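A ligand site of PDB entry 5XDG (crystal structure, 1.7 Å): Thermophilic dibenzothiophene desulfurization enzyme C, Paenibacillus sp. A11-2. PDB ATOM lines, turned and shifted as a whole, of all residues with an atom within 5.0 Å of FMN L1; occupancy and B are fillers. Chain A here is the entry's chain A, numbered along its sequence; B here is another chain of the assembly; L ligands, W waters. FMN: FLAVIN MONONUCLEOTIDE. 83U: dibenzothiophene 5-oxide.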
ATOM      1  N   HIS A  89     -17.280 -32.708  -5.008  1.00  0.00           N
ATOM      2  CA  HIS A  89     -17.056 -31.270  -4.851  1.00  0.00           C
ATOM      3  C   HIS A  89     -15.804 -30.831  -5.603  1.00  0.00           C
ATOM      4  O   HIS A  89     -15.846 -29.864  -6.377  1.00  0.00           O
ATOM      5  CB  HIS A  89     -16.956 -30.949  -3.366  1.00  0.00           C
ATOM      6  CG  HIS A  89     -16.541 -29.545  -3.055  1.00  0.00           C
ATOM      7  ND1 HIS A  89     -17.390 -28.626  -2.493  1.00  0.00           N
ATOM      8  CD2 HIS A  89     -15.331 -28.932  -3.157  1.00  0.00           C
ATOM      9  CE1 HIS A  89     -16.749 -27.490  -2.291  1.00  0.00           C
ATOM     10  NE2 HIS A  89     -15.500 -27.649  -2.706  1.00  0.00           N
ATOM     11  N   TYR A  93     -15.937 -28.373  -8.702  1.00  0.00           N
ATOM     12  CA  TYR A  93     -15.310 -27.051  -8.663  1.00  0.00           C
ATOM     13  C   TYR A  93     -14.260 -26.909  -9.753  1.00  0.00           C
ATOM     14  O   TYR A  93     -14.059 -25.808 -10.283  1.00  0.00           O
ATOM     15  CB  TYR A  93     -14.667 -26.796  -7.309  1.00  0.00           C
ATOM     16  CG  TYR A  93     -15.646 -26.285  -6.284  1.00  0.00           C
ATOM     17  CD1 TYR A  93     -15.460 -25.053  -5.662  1.00  0.00           C
ATOM     18  CD2 TYR A  93     -16.779 -27.016  -5.968  1.00  0.00           C
ATOM     19  CE1 TYR A  93     -16.367 -24.583  -4.718  1.00  0.00           C
ATOM     20  CE2 TYR A  93     -17.684 -26.565  -5.044  1.00  0.00           C
ATOM     21  CZ  TYR A  93     -17.472 -25.347  -4.415  1.00  0.00           C
ATOM     22  OH  TYR A  93     -18.394 -24.901  -3.478  1.00  0.00           O
ATOM     23  N   ASN A 126      -9.099 -23.066  -6.623  1.00  0.00           N
ATOM     24  CA  ASN A 126      -9.321 -21.633  -6.653  1.00  0.00           C
ATOM     25  C   ASN A 126      -9.088 -21.024  -5.285  1.00  0.00           C
ATOM     26  O   ASN A 126      -9.197 -21.685  -4.253  1.00  0.00           O
ATOM     27  CB  ASN A 126     -10.730 -21.294  -7.148  1.00  0.00           C
ATOM     28  CG  ASN A 126     -11.768 -21.443  -6.060  1.00  0.00           C
ATOM     29  OD1 ASN A 126     -12.144 -20.469  -5.398  1.00  0.00           O
ATOM     30  ND2 ASN A 126     -12.213 -22.678  -5.855  1.00  0.00           N
ATOM     31  N   SER A 128     -10.569 -17.463  -3.880  1.00  0.00           N
ATOM     32  CA  SER A 128     -11.469 -16.375  -4.296  1.00  0.00           C
ATOM     33  C   SER A 128     -12.127 -15.654  -3.121  1.00  0.00           C
ATOM     34  O   SER A 128     -11.980 -14.434  -2.978  1.00  0.00           O
ATOM     35  CB  SER A 128     -12.550 -16.933  -5.224  1.00  0.00           C
ATOM     36  OG  SER A 128     -12.015 -17.912  -6.091  1.00  0.00           O
ATOM     37  N   SER A 129     -12.879 -16.383  -2.306  1.00  0.00           N
ATOM     38  CA  SER A 129     -13.601 -15.771  -1.200  1.00  0.00           C
ATOM     39  C   SER A 129     -12.655 -15.461  -0.033  1.00  0.00           C
ATOM     40  O   SER A 129     -11.492 -15.869  -0.026  1.00  0.00           O
ATOM     41  CB  SER A 129     -14.745 -16.684  -0.737  1.00  0.00           C
ATOM     42  OG  SER A 129     -15.749 -16.795  -1.727  1.00  0.00           O
ATOM     43  N   GLU A 130     -13.168 -14.728   0.947  1.00  0.00           N
ATOM     44  CA  GLU A 130     -12.354 -14.277   2.059  1.00  0.00           C
ATOM     45  C   GLU A 130     -13.151 -14.426   3.355  1.00  0.00           C
ATOM     46  O   GLU A 130     -14.338 -14.771   3.337  1.00  0.00           O
ATOM     47  CB  GLU A 130     -11.868 -12.823   1.833  1.00  0.00           C
ATOM     48  CG  GLU A 130     -10.953 -12.726   0.603  1.00  0.00           C
ATOM     49  CD  GLU A 130     -10.368 -11.338   0.353  1.00  0.00           C
ATOM     50  OE1 GLU A 130     -10.092 -11.033  -0.838  1.00  0.00           O
ATOM     51  OE2 GLU A 130     -10.168 -10.575   1.318  1.00  0.00           O
ATOM     52  N   VAL A 135     -19.331 -11.154   2.959  1.00  0.00           N
ATOM     53  CA  VAL A 135     -18.759 -11.742   1.744  1.00  0.00           C
ATOM     54  C   VAL A 135     -18.270 -10.687   0.757  1.00  0.00           C
ATOM     55  O   VAL A 135     -17.472 -10.992  -0.123  1.00  0.00           O
ATOM     56  CB  VAL A 135     -19.737 -12.701   1.031  1.00  0.00           C
ATOM     57  CG1 VAL A 135     -19.871 -14.018   1.808  1.00  0.00           C
ATOM     58  CG2 VAL A 135     -21.089 -12.031   0.813  1.00  0.00           C
ATOM     59  N   ALA A 157      -9.932 -17.405   1.819  1.00  0.00           N
ATOM     60  CA  ALA A 157     -10.582 -18.437   2.616  1.00  0.00           C
ATOM     61  C   ALA A 157     -11.372 -19.362   1.693  1.00  0.00           C
ATOM     62  O   ALA A 157     -11.639 -19.041   0.542  1.00  0.00           O
ATOM     63  CB  ALA A 157     -11.500 -17.827   3.670  1.00  0.00           C
ATOM     64  N   PHE A 158     -11.729 -20.538   2.227  1.00  0.00           N
ATOM     65  CA  PHE A 158     -12.523 -21.530   1.498  1.00  0.00           C
ATOM     66  C   PHE A 158     -11.934 -21.820   0.112  1.00  0.00           C
ATOM     67  O   PHE A 158     -12.614 -21.759  -0.921  1.00  0.00           O
ATOM     68  CB  PHE A 158     -13.985 -21.088   1.382  1.00  0.00           C
ATOM     69  CG  PHE A 158     -14.772 -21.203   2.665  1.00  0.00           C
ATOM     70  CD1 PHE A 158     -15.247 -22.430   3.097  1.00  0.00           C
ATOM     71  CD2 PHE A 158     -15.052 -20.070   3.420  1.00  0.00           C
ATOM     72  CE1 PHE A 158     -15.977 -22.537   4.280  1.00  0.00           C
ATOM     73  CE2 PHE A 158     -15.792 -20.180   4.604  1.00  0.00           C
ATOM     74  CZ  PHE A 158     -16.256 -21.414   5.025  1.00  0.00           C
ATOM     75  N   CYS A 159     -10.638 -22.160   0.078  1.00  0.00           N
ATOM     76  CA  CYS A 159      -9.944 -22.350  -1.194  1.00  0.00           C
ATOM     77  C   CYS A 159     -10.032 -23.807  -1.654  1.00  0.00           C
ATOM     78  O   CYS A 159      -9.070 -24.571  -1.619  1.00  0.00           O
ATOM     79  CB  CYS A 159      -8.489 -21.892  -1.077  1.00  0.00           C
ATOM     80  SG  CYS A 159      -8.378 -20.159  -0.647  1.00  0.00           S
ATOM     81  N   SER A 160     -11.227 -24.178  -2.105  1.00  0.00           N
ATOM     82  CA  SER A 160     -11.477 -25.578  -2.431  1.00  0.00           C
ATOM     83  C   SER A 160     -10.453 -26.088  -3.432  1.00  0.00           C
ATOM     84  O   SER A 160     -10.149 -25.437  -4.432  1.00  0.00           O
ATOM     85  CB  SER A 160     -12.882 -25.755  -3.007  1.00  0.00           C
ATOM     86  OG  SER A 160     -13.847 -25.706  -1.974  1.00  0.00           O
ATOM     87  N   TRP A 202      -8.195 -26.895   6.909  1.00  0.00           N
ATOM     88  CA  TRP A 202      -9.572 -27.351   6.689  1.00  0.00           C
ATOM     89  C   TRP A 202      -9.906 -28.497   7.634  1.00  0.00           C
ATOM     90  O   TRP A 202      -9.308 -29.576   7.539  1.00  0.00           O
ATOM     91  CB  TRP A 202      -9.754 -27.778   5.229  1.00  0.00           C
ATOM     92  CG  TRP A 202     -11.165 -28.168   4.841  1.00  0.00           C
ATOM     93  CD1 TRP A 202     -11.568 -29.378   4.342  1.00  0.00           C
ATOM     94  CD2 TRP A 202     -12.343 -27.340   4.877  1.00  0.00           C
ATOM     95  NE1 TRP A 202     -12.925 -29.361   4.078  1.00  0.00           N
ATOM     96  CE2 TRP A 202     -13.418 -28.123   4.397  1.00  0.00           C
ATOM     97  CE3 TRP A 202     -12.586 -26.014   5.268  1.00  0.00           C
ATOM     98  CZ2 TRP A 202     -14.724 -27.628   4.298  1.00  0.00           C
ATOM     99  CZ3 TRP A 202     -13.880 -25.526   5.167  1.00  0.00           C
ATOM    100  CH2 TRP A 202     -14.939 -26.326   4.695  1.00  0.00           C
ATOM    101  N   MET A 207     -17.801 -32.481   4.146  1.00  0.00           N
ATOM    102  CA  MET A 207     -16.925 -32.096   3.036  1.00  0.00           C
ATOM    103  C   MET A 207     -15.474 -32.029   3.516  1.00  0.00           C
ATOM    104  O   MET A 207     -14.720 -31.112   3.181  1.00  0.00           O
ATOM    105  CB  MET A 207     -17.420 -30.778   2.403  1.00  0.00           C
ATOM    106  CG  MET A 207     -18.801 -30.946   1.652  1.00  0.00           C
ATOM    107  SD  MET A 207     -18.626 -31.980   0.192  1.00  0.00           S
ATOM    108  CE  MET A 207     -20.057 -31.503  -0.808  1.00  0.00           C
ATOM    109  N   THR A 210     -12.172 -31.722   1.005  1.00  0.00           N
ATOM    110  CA  THR A 210     -12.181 -30.740  -0.077  1.00  0.00           C
ATOM    111  C   THR A 210     -11.015 -29.748   0.010  1.00  0.00           C
ATOM    112  O   THR A 210     -10.818 -28.982  -0.936  1.00  0.00           O
ATOM    113  CB  THR A 210     -13.495 -29.948  -0.101  1.00  0.00           C
ATOM    114  OG1 THR A 210     -13.659 -29.207   1.110  1.00  0.00           O
ATOM    115  CG2 THR A 210     -14.678 -30.891  -0.278  1.00  0.00           C
ATOM    116  N   SER A 212     -10.723 -27.063   1.545  1.00  0.00           N
ATOM    117  CA  SER A 212     -11.202 -25.689   1.444  1.00  0.00           C
ATOM    118  C   SER A 212     -10.718 -24.821   2.597  1.00  0.00           C
ATOM    119  O   SER A 212     -11.489 -24.057   3.180  1.00  0.00           O
ATOM    120  CB  SER A 212     -12.733 -25.692   1.379  1.00  0.00           C
ATOM    121  OG  SER A 212     -13.207 -26.655   0.460  1.00  0.00           O
ATOM    122  N   THR A 384     -23.090 -29.225   5.478  1.00  0.00           N
ATOM    123  CA  THR A 384     -21.973 -28.284   5.362  1.00  0.00           C
ATOM    124  C   THR A 384     -22.066 -27.498   4.064  1.00  0.00           C
ATOM    125  O   THR A 384     -21.988 -26.263   4.065  1.00  0.00           O
ATOM    126  CB  THR A 384     -20.639 -29.040   5.443  1.00  0.00           C
ATOM    127  OG1 THR A 384     -20.521 -29.654   6.733  1.00  0.00           O
ATOM    128  CG2 THR A 384     -19.470 -28.084   5.217  1.00  0.00           C
ATOM    129  N   HIS A 385     -22.259 -28.193   2.935  1.00  0.00           N
ATOM    130  CA  HIS A 385     -22.147 -27.486   1.669  1.00  0.00           C
ATOM    131  C   HIS A 385     -23.358 -26.619   1.365  1.00  0.00           C
ATOM    132  O   HIS A 385     -23.221 -25.574   0.724  1.00  0.00           O
ATOM    133  CB  HIS A 385     -21.934 -28.453   0.506  1.00  0.00           C
ATOM    134  CG  HIS A 385     -21.451 -27.780  -0.724  1.00  0.00           C
ATOM    135  ND1 HIS A 385     -22.280 -27.017  -1.528  1.00  0.00           N
ATOM    136  CD2 HIS A 385     -20.210 -27.679  -1.265  1.00  0.00           C
ATOM    137  CE1 HIS A 385     -21.571 -26.494  -2.515  1.00  0.00           C
ATOM    138  NE2 HIS A 385     -20.319 -26.890  -2.389  1.00  0.00           N
ATOM    139  N   LEU A 387     -24.866 -24.605   3.011  1.00  0.00           N
ATOM    140  CA  LEU A 387     -24.715 -23.278   3.576  1.00  0.00           C
ATOM    141  C   LEU A 387     -23.775 -22.404   2.739  1.00  0.00           C
ATOM    142  O   LEU A 387     -23.589 -21.240   3.110  1.00  0.00           O
ATOM    143  CB  LEU A 387     -24.183 -23.376   5.005  1.00  0.00           C
ATOM    144  CG  LEU A 387     -24.918 -24.321   5.955  1.00  0.00           C
ATOM    145  CD1 LEU A 387     -24.051 -24.624   7.147  1.00  0.00           C
ATOM    146  CD2 LEU A 387     -26.252 -23.688   6.392  1.00  0.00           C
ATOM    147  N   HIS A 388     -23.209 -22.934   1.655  1.00  0.00           N
ATOM    148  CA  HIS A 388     -22.331 -22.179   0.749  1.00  0.00           C
ATOM    149  C   HIS A 388     -22.832 -20.757   0.529  1.00  0.00           C
ATOM    150  O   HIS A 388     -22.126 -19.780   0.806  1.00  0.00           O
ATOM    151  CB  HIS A 388     -22.231 -22.915  -0.595  1.00  0.00           C
ATOM    152  CG  HIS A 388     -21.037 -22.531  -1.408  1.00  0.00           C
ATOM    153  ND1 HIS A 388     -20.990 -21.384  -2.169  1.00  0.00           N
ATOM    154  CD2 HIS A 388     -19.856 -23.158  -1.611  1.00  0.00           C
ATOM    155  CE1 HIS A 388     -19.817 -21.301  -2.780  1.00  0.00           C
ATOM    156  NE2 HIS A 388     -19.112 -22.379  -2.457  1.00  0.00           N
ATOM    157  N   TYR A 413     -22.699 -14.584  -7.152  1.00  0.00           N
ATOM    158  CA  TYR A 413     -23.638 -15.456  -6.437  1.00  0.00           C
ATOM    159  C   TYR A 413     -25.042 -15.487  -7.026  1.00  0.00           C
ATOM    160  O   TYR A 413     -25.859 -16.300  -6.573  1.00  0.00           O
ATOM    161  CB  TYR A 413     -23.742 -15.045  -4.954  1.00  0.00           C
ATOM    162  CG  TYR A 413     -22.430 -14.720  -4.237  1.00  0.00           C
ATOM    163  CD1 TYR A 413     -21.887 -15.574  -3.277  1.00  0.00           C
ATOM    164  CD2 TYR A 413     -21.760 -13.526  -4.484  1.00  0.00           C
ATOM    165  CE1 TYR A 413     -20.715 -15.266  -2.609  1.00  0.00           C
ATOM    166  CE2 TYR A 413     -20.573 -13.203  -3.829  1.00  0.00           C
ATOM    167  CZ  TYR A 413     -20.059 -14.075  -2.885  1.00  0.00           C
ATOM    168  OH  TYR A 413     -18.885 -13.745  -2.238  1.00  0.00           O
ATOM    169  N   ARG B 279     -22.356 -13.627  10.088  1.00  0.00           N
ATOM    170  CA  ARG B 279     -22.137 -12.393   9.371  1.00  0.00           C
ATOM    171  C   ARG B 279     -23.388 -11.995   8.577  1.00  0.00           C
ATOM    172  O   ARG B 279     -24.117 -12.859   8.088  1.00  0.00           O
ATOM    173  CB  ARG B 279     -20.956 -12.508   8.398  1.00  0.00           C
ATOM    174  CG  ARG B 279     -19.698 -13.057   9.032  1.00  0.00           C
ATOM    175  CD  ARG B 279     -19.066 -14.101   8.132  1.00  0.00           C
ATOM    176  NE  ARG B 279     -18.073 -13.532   7.233  1.00  0.00           N
ATOM    177  CZ  ARG B 279     -17.642 -14.120   6.120  1.00  0.00           C
ATOM    178  NH1 ARG B 279     -18.128 -15.294   5.764  1.00  0.00           N
ATOM    179  NH2 ARG B 279     -16.715 -13.531   5.372  1.00  0.00           N
ATOM    180  N   MET B 363     -27.253 -19.814  11.380  1.00  0.00           N
ATOM    181  CA  MET B 363     -25.896 -19.533  11.839  1.00  0.00           C
ATOM    182  C   MET B 363     -24.914 -19.275  10.716  1.00  0.00           C
ATOM    183  O   MET B 363     -24.071 -18.383  10.844  1.00  0.00           O
ATOM    184  CB  MET B 363     -25.389 -20.686  12.710  1.00  0.00           C
ATOM    185  CG  MET B 363     -26.139 -20.875  14.029  1.00  0.00           C
ATOM    186  SD  MET B 363     -25.405 -22.155  15.061  1.00  0.00           S
ATOM    187  CE  MET B 363     -26.158 -23.635  14.397  1.00  0.00           C
ATOM    188  N   GLY B 364     -24.974 -20.018   9.609  1.00  0.00           N
ATOM    189  CA  GLY B 364     -24.114 -19.782   8.475  1.00  0.00           C
ATOM    190  C   GLY B 364     -23.046 -20.855   8.309  1.00  0.00           C
ATOM    191  O   GLY B 364     -22.814 -21.690   9.193  1.00  0.00           O
ATOM    192  N   ALA B 365     -22.389 -20.810   7.148  1.00  0.00           N
ATOM    193  CA  ALA B 365     -21.463 -21.876   6.751  1.00  0.00           C
ATOM    194  C   ALA B 365     -20.380 -22.138   7.789  1.00  0.00           C
ATOM    195  O   ALA B 365     -19.953 -23.279   7.963  1.00  0.00           O
ATOM    196  CB  ALA B 365     -20.821 -21.540   5.404  1.00  0.00           C
ATOM    197  N   ARG B 366     -19.913 -21.090   8.475  1.00  0.00           N
ATOM    198  CA  ARG B 366     -18.782 -21.295   9.383  1.00  0.00           C
ATOM    199  C   ARG B 366     -19.169 -22.077  10.631  1.00  0.00           C
ATOM    200  O   ARG B 366     -18.278 -22.603  11.309  1.00  0.00           O
ATOM    201  CB  ARG B 366     -18.169 -19.941   9.726  1.00  0.00           C
ATOM    202  CG  ARG B 366     -17.381 -19.351   8.554  1.00  0.00           C
ATOM    203  CD  ARG B 366     -17.488 -17.833   8.476  1.00  0.00           C
ATOM    204  NE  ARG B 366     -17.125 -17.187   9.732  1.00  0.00           N
ATOM    205  CZ  ARG B 366     -17.965 -16.498  10.489  1.00  0.00           C
ATOM    206  NH1 ARG B 366     -19.236 -16.362  10.109  1.00  0.00           N
ATOM    207  NH2 ARG B 366     -17.555 -15.940  11.619  1.00  0.00           N
HETATM  208  N1  FMN L   1     -15.893 -19.913  -1.788  1.00  0.00           N
HETATM  209  C2  FMN L   1     -15.055 -19.716  -2.868  1.00  0.00           C
HETATM  210  O2  FMN L   1     -14.871 -18.569  -3.285  1.00  0.00           O
HETATM  211  N3  FMN L   1     -14.434 -20.789  -3.483  1.00  0.00           N
HETATM  212  C4  FMN L   1     -14.644 -22.079  -3.008  1.00  0.00           C
HETATM  213  O4  FMN L   1     -14.075 -23.033  -3.547  1.00  0.00           O
HETATM  214  C4A FMN L   1     -15.489 -22.279  -1.917  1.00  0.00           C
HETATM  215  N5  FMN L   1     -15.691 -23.566  -1.454  1.00  0.00           N
HETATM  216  C5A FMN L   1     -16.523 -23.783  -0.374  1.00  0.00           C
HETATM  217  C6  FMN L   1     -16.742 -25.075   0.102  1.00  0.00           C
HETATM  218  C7  FMN L   1     -17.586 -25.316   1.194  1.00  0.00           C
HETATM  219  C7M FMN L   1     -17.814 -26.705   1.714  1.00  0.00           C
HETATM  220  C8  FMN L   1     -18.202 -24.231   1.797  1.00  0.00           C
HETATM  221  C8M FMN L   1     -19.130 -24.351   2.970  1.00  0.00           C
HETATM  222  C9  FMN L   1     -17.990 -22.951   1.323  1.00  0.00           C
HETATM  223  C9A FMN L   1     -17.149 -22.690   0.241  1.00  0.00           C
HETATM  224  N10 FMN L   1     -16.984 -21.392  -0.237  1.00  0.00           N
HETATM  225  C10 FMN L   1     -16.115 -21.186  -1.302  1.00  0.00           C
HETATM  226  C1' FMN L   1     -17.611 -20.219   0.518  1.00  0.00           C
HETATM  227  C2' FMN L   1     -18.851 -19.422   0.169  1.00  0.00           C
HETATM  228  O2' FMN L   1     -18.701 -18.818  -1.101  1.00  0.00           O
HETATM  229  C3' FMN L   1     -19.008 -18.345   1.281  1.00  0.00           C
HETATM  230  O3' FMN L   1     -17.887 -17.487   1.246  1.00  0.00           O
HETATM  231  C4' FMN L   1     -19.154 -18.867   2.720  1.00  0.00           C
HETATM  232  O4' FMN L   1     -19.789 -20.129   2.670  1.00  0.00           O
HETATM  233  C5' FMN L   1     -19.928 -17.925   3.674  1.00  0.00           C
HETATM  234  O5' FMN L   1     -19.704 -18.190   5.052  1.00  0.00           O
HETATM  235  P   FMN L   1     -20.769 -17.746   6.212  1.00  0.00           P
HETATM  236  O1P FMN L   1     -22.156 -18.201   5.792  1.00  0.00           O
HETATM  237  O2P FMN L   1     -20.454 -18.410   7.535  1.00  0.00           O
HETATM  238  O3P FMN L   1     -20.749 -16.251   6.438  1.00  0.00           O
HETATM  239  C4  83U L   2     -17.126 -18.282  -5.615  1.00  0.00           C
HETATM  240  C7  83U L   2     -16.268 -21.478  -6.865  1.00  0.00           C
HETATM  241  C1  83U L   2     -15.628 -19.152  -7.042  1.00  0.00           C
HETATM  242  O1  83U L   2     -18.754 -19.974  -6.073  1.00  0.00           O
HETATM  243  C10 83U L   2     -16.455 -15.637  -5.835  1.00  0.00           C
HETATM  244  S1  83U L   2     -17.389 -19.693  -5.565  1.00  0.00           S
HETATM  245  C2  83U L   2     -16.087 -17.920  -6.455  1.00  0.00           C
HETATM  246  C3  83U L   2     -16.421 -20.157  -6.507  1.00  0.00           C
HETATM  247  C5  83U L   2     -14.650 -19.490  -7.969  1.00  0.00           C
HETATM  248  C6  83U L   2     -15.752 -16.582  -6.575  1.00  0.00           C
HETATM  249  C8  83U L   2     -17.834 -17.360  -4.883  1.00  0.00           C
HETATM  250  C9  83U L   2     -14.486 -20.817  -8.328  1.00  0.00           C
HETATM  251  C11 83U L   2     -15.291 -21.805  -7.772  1.00  0.00           C
HETATM  252  C12 83U L   2     -17.486 -16.028  -4.995  1.00  0.00           C
HETATM  253  O   HOH W   1     -17.742 -15.570  -1.033  1.00  0.00           O
HETATM  254  O   HOH W   2     -24.172 -16.549   5.479  1.00  0.00           O
HETATM  255  O   HOH W   3     -22.269 -16.376   1.894  1.00  0.00           O
HETATM  256  O   HOH W   4     -16.431 -16.469   3.049  1.00  0.00           O
HETATM  257  O   HOH W   5     -22.563 -14.689   4.429  1.00  0.00           O
HETATM  258  O   HOH W   6     -21.540 -18.496  10.116  1.00  0.00           O
HETATM  259  O   HOH W   7     -12.073 -19.423  -2.055  1.00  0.00           O
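An oxygen (O4) of FMN L1 sits close to the backbone NH of Ser 160.
An oxygen (O2) of FMN L1 sits at hydrogen-bond distance from the side-chain hydroxyl (OG) of Ser 129 (2.5 Å).
An oxygen (O2P) of FMN L1 is in salt-bridge range of the guanidinium group (NH1) of Arg 366 of chain B.
An oxygen (O1P) of FMN L1 is in hydrogen-bond range of the backbone NH (N) of Ala 365 of chain B, 2.9 Å away.
N3 of FMN L1 sits close to O of Phe 158, at 3.3 Å.
N of Ser 129 is in hydrogen-bond range of O2 of FMN L1, at 3.1 Å.
The backbone carbonyl oxygen (O) of His 388 is in hydrogen-bond range of an oxygen (O4') of FMN L1 (3.0 Å).
The side-chain hydroxyl of Ser 160 is in hydrogen-bond range of a nitrogen (N5) of FMN L1 (2.9 Å).
O4 of FMN L1 lies within hydrogen-bond range of ND2 of Asn 126, at 3.0 Å.
An oxygen (O2P) of FMN L1 sits at hydrogen-bond distance from the backbone NH (N) of Arg 366 of chain B, 2.9 Å away.
NH1 of Arg 279 of chain B lies within salt-bridge range of O3P of FMN L1, at 2.9 Å.
The side-chain hydroxyl of Ser 160 sits at hydrogen-bond distance from the side-chain hydroxyl of Ser 212, 2.7 Å away.
A ring nitrogen (NE2) of His 385 sits at hydrogen-bond distance from the side-chain hydroxyl (OH) of Tyr 93 (3.0 Å).
The side-chain amide oxygen (OD1) of Asn 126 sits at hydrogen-bond distance from the side-chain hydroxyl (OG) of Ser 128 (2.7 Å).
The backbone carbonyl oxygen (O) of Glu 130 lies within hydrogen-bond range of the guanidinium group (NH2) of Arg 279 of chain B, 3.4 Å away.
NE2 of His 388 sits at hydrogen-bond distance from OH of Tyr 93 (2.8 Å).
O of Ser 129 sits at hydrogen-bond distance from N of Ala 157 (2.9 Å).
OG of Ser 160 is in hydrogen-bond range of NE2 of His 89, at 2.7 Å.
NE2 of His 385 sits close to ND1 of His 89 (3.4 Å).
CE1 of His 89 touches C6 of FMN L1 (3.4 Å).
Tyr 93 touches FMN L1.
Ser 128 touches FMN L1 (CB to O2, 3.4 Å).
Ser 212 touches FMN L1.
O of Thr 384 touches C8M of FMN L1, 3.6 Å away.
CD2 of His 385 touches C7M of FMN L1, at 3.9 Å.
Leu 387 touches FMN L1.
Gly 364 of chain B touches FMN L1 (C to O2P, 3.6 Å).
Within 4 Å of FMN L1: His 89, Tyr 93, Asn 126, Ser 128, Ser 129, Phe 158, Ser 160, Ser 212, Thr 384, His 385, Leu 387, His 388, Arg 279 of chain B, Gly 364 of chain B, Ala 365 of chain B and Arg 366 of chain B.
Water W4 lies within hydrogen-bond range of an oxygen (O3') of FMN L1, the backbone carbonyl oxygen (O) of Glu 130 and the guanidinium group (NH1) of Arg 279 of chain B.
Water W6 lies within hydrogen-bond range of O of Met 363 of chain B, O2P of FMN L1 and NH1 of Arg 366 of chain B.
Water W1 lies within hydrogen-bond range of OG of Ser 129, OH of Tyr 413 and O3' of FMN L1.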
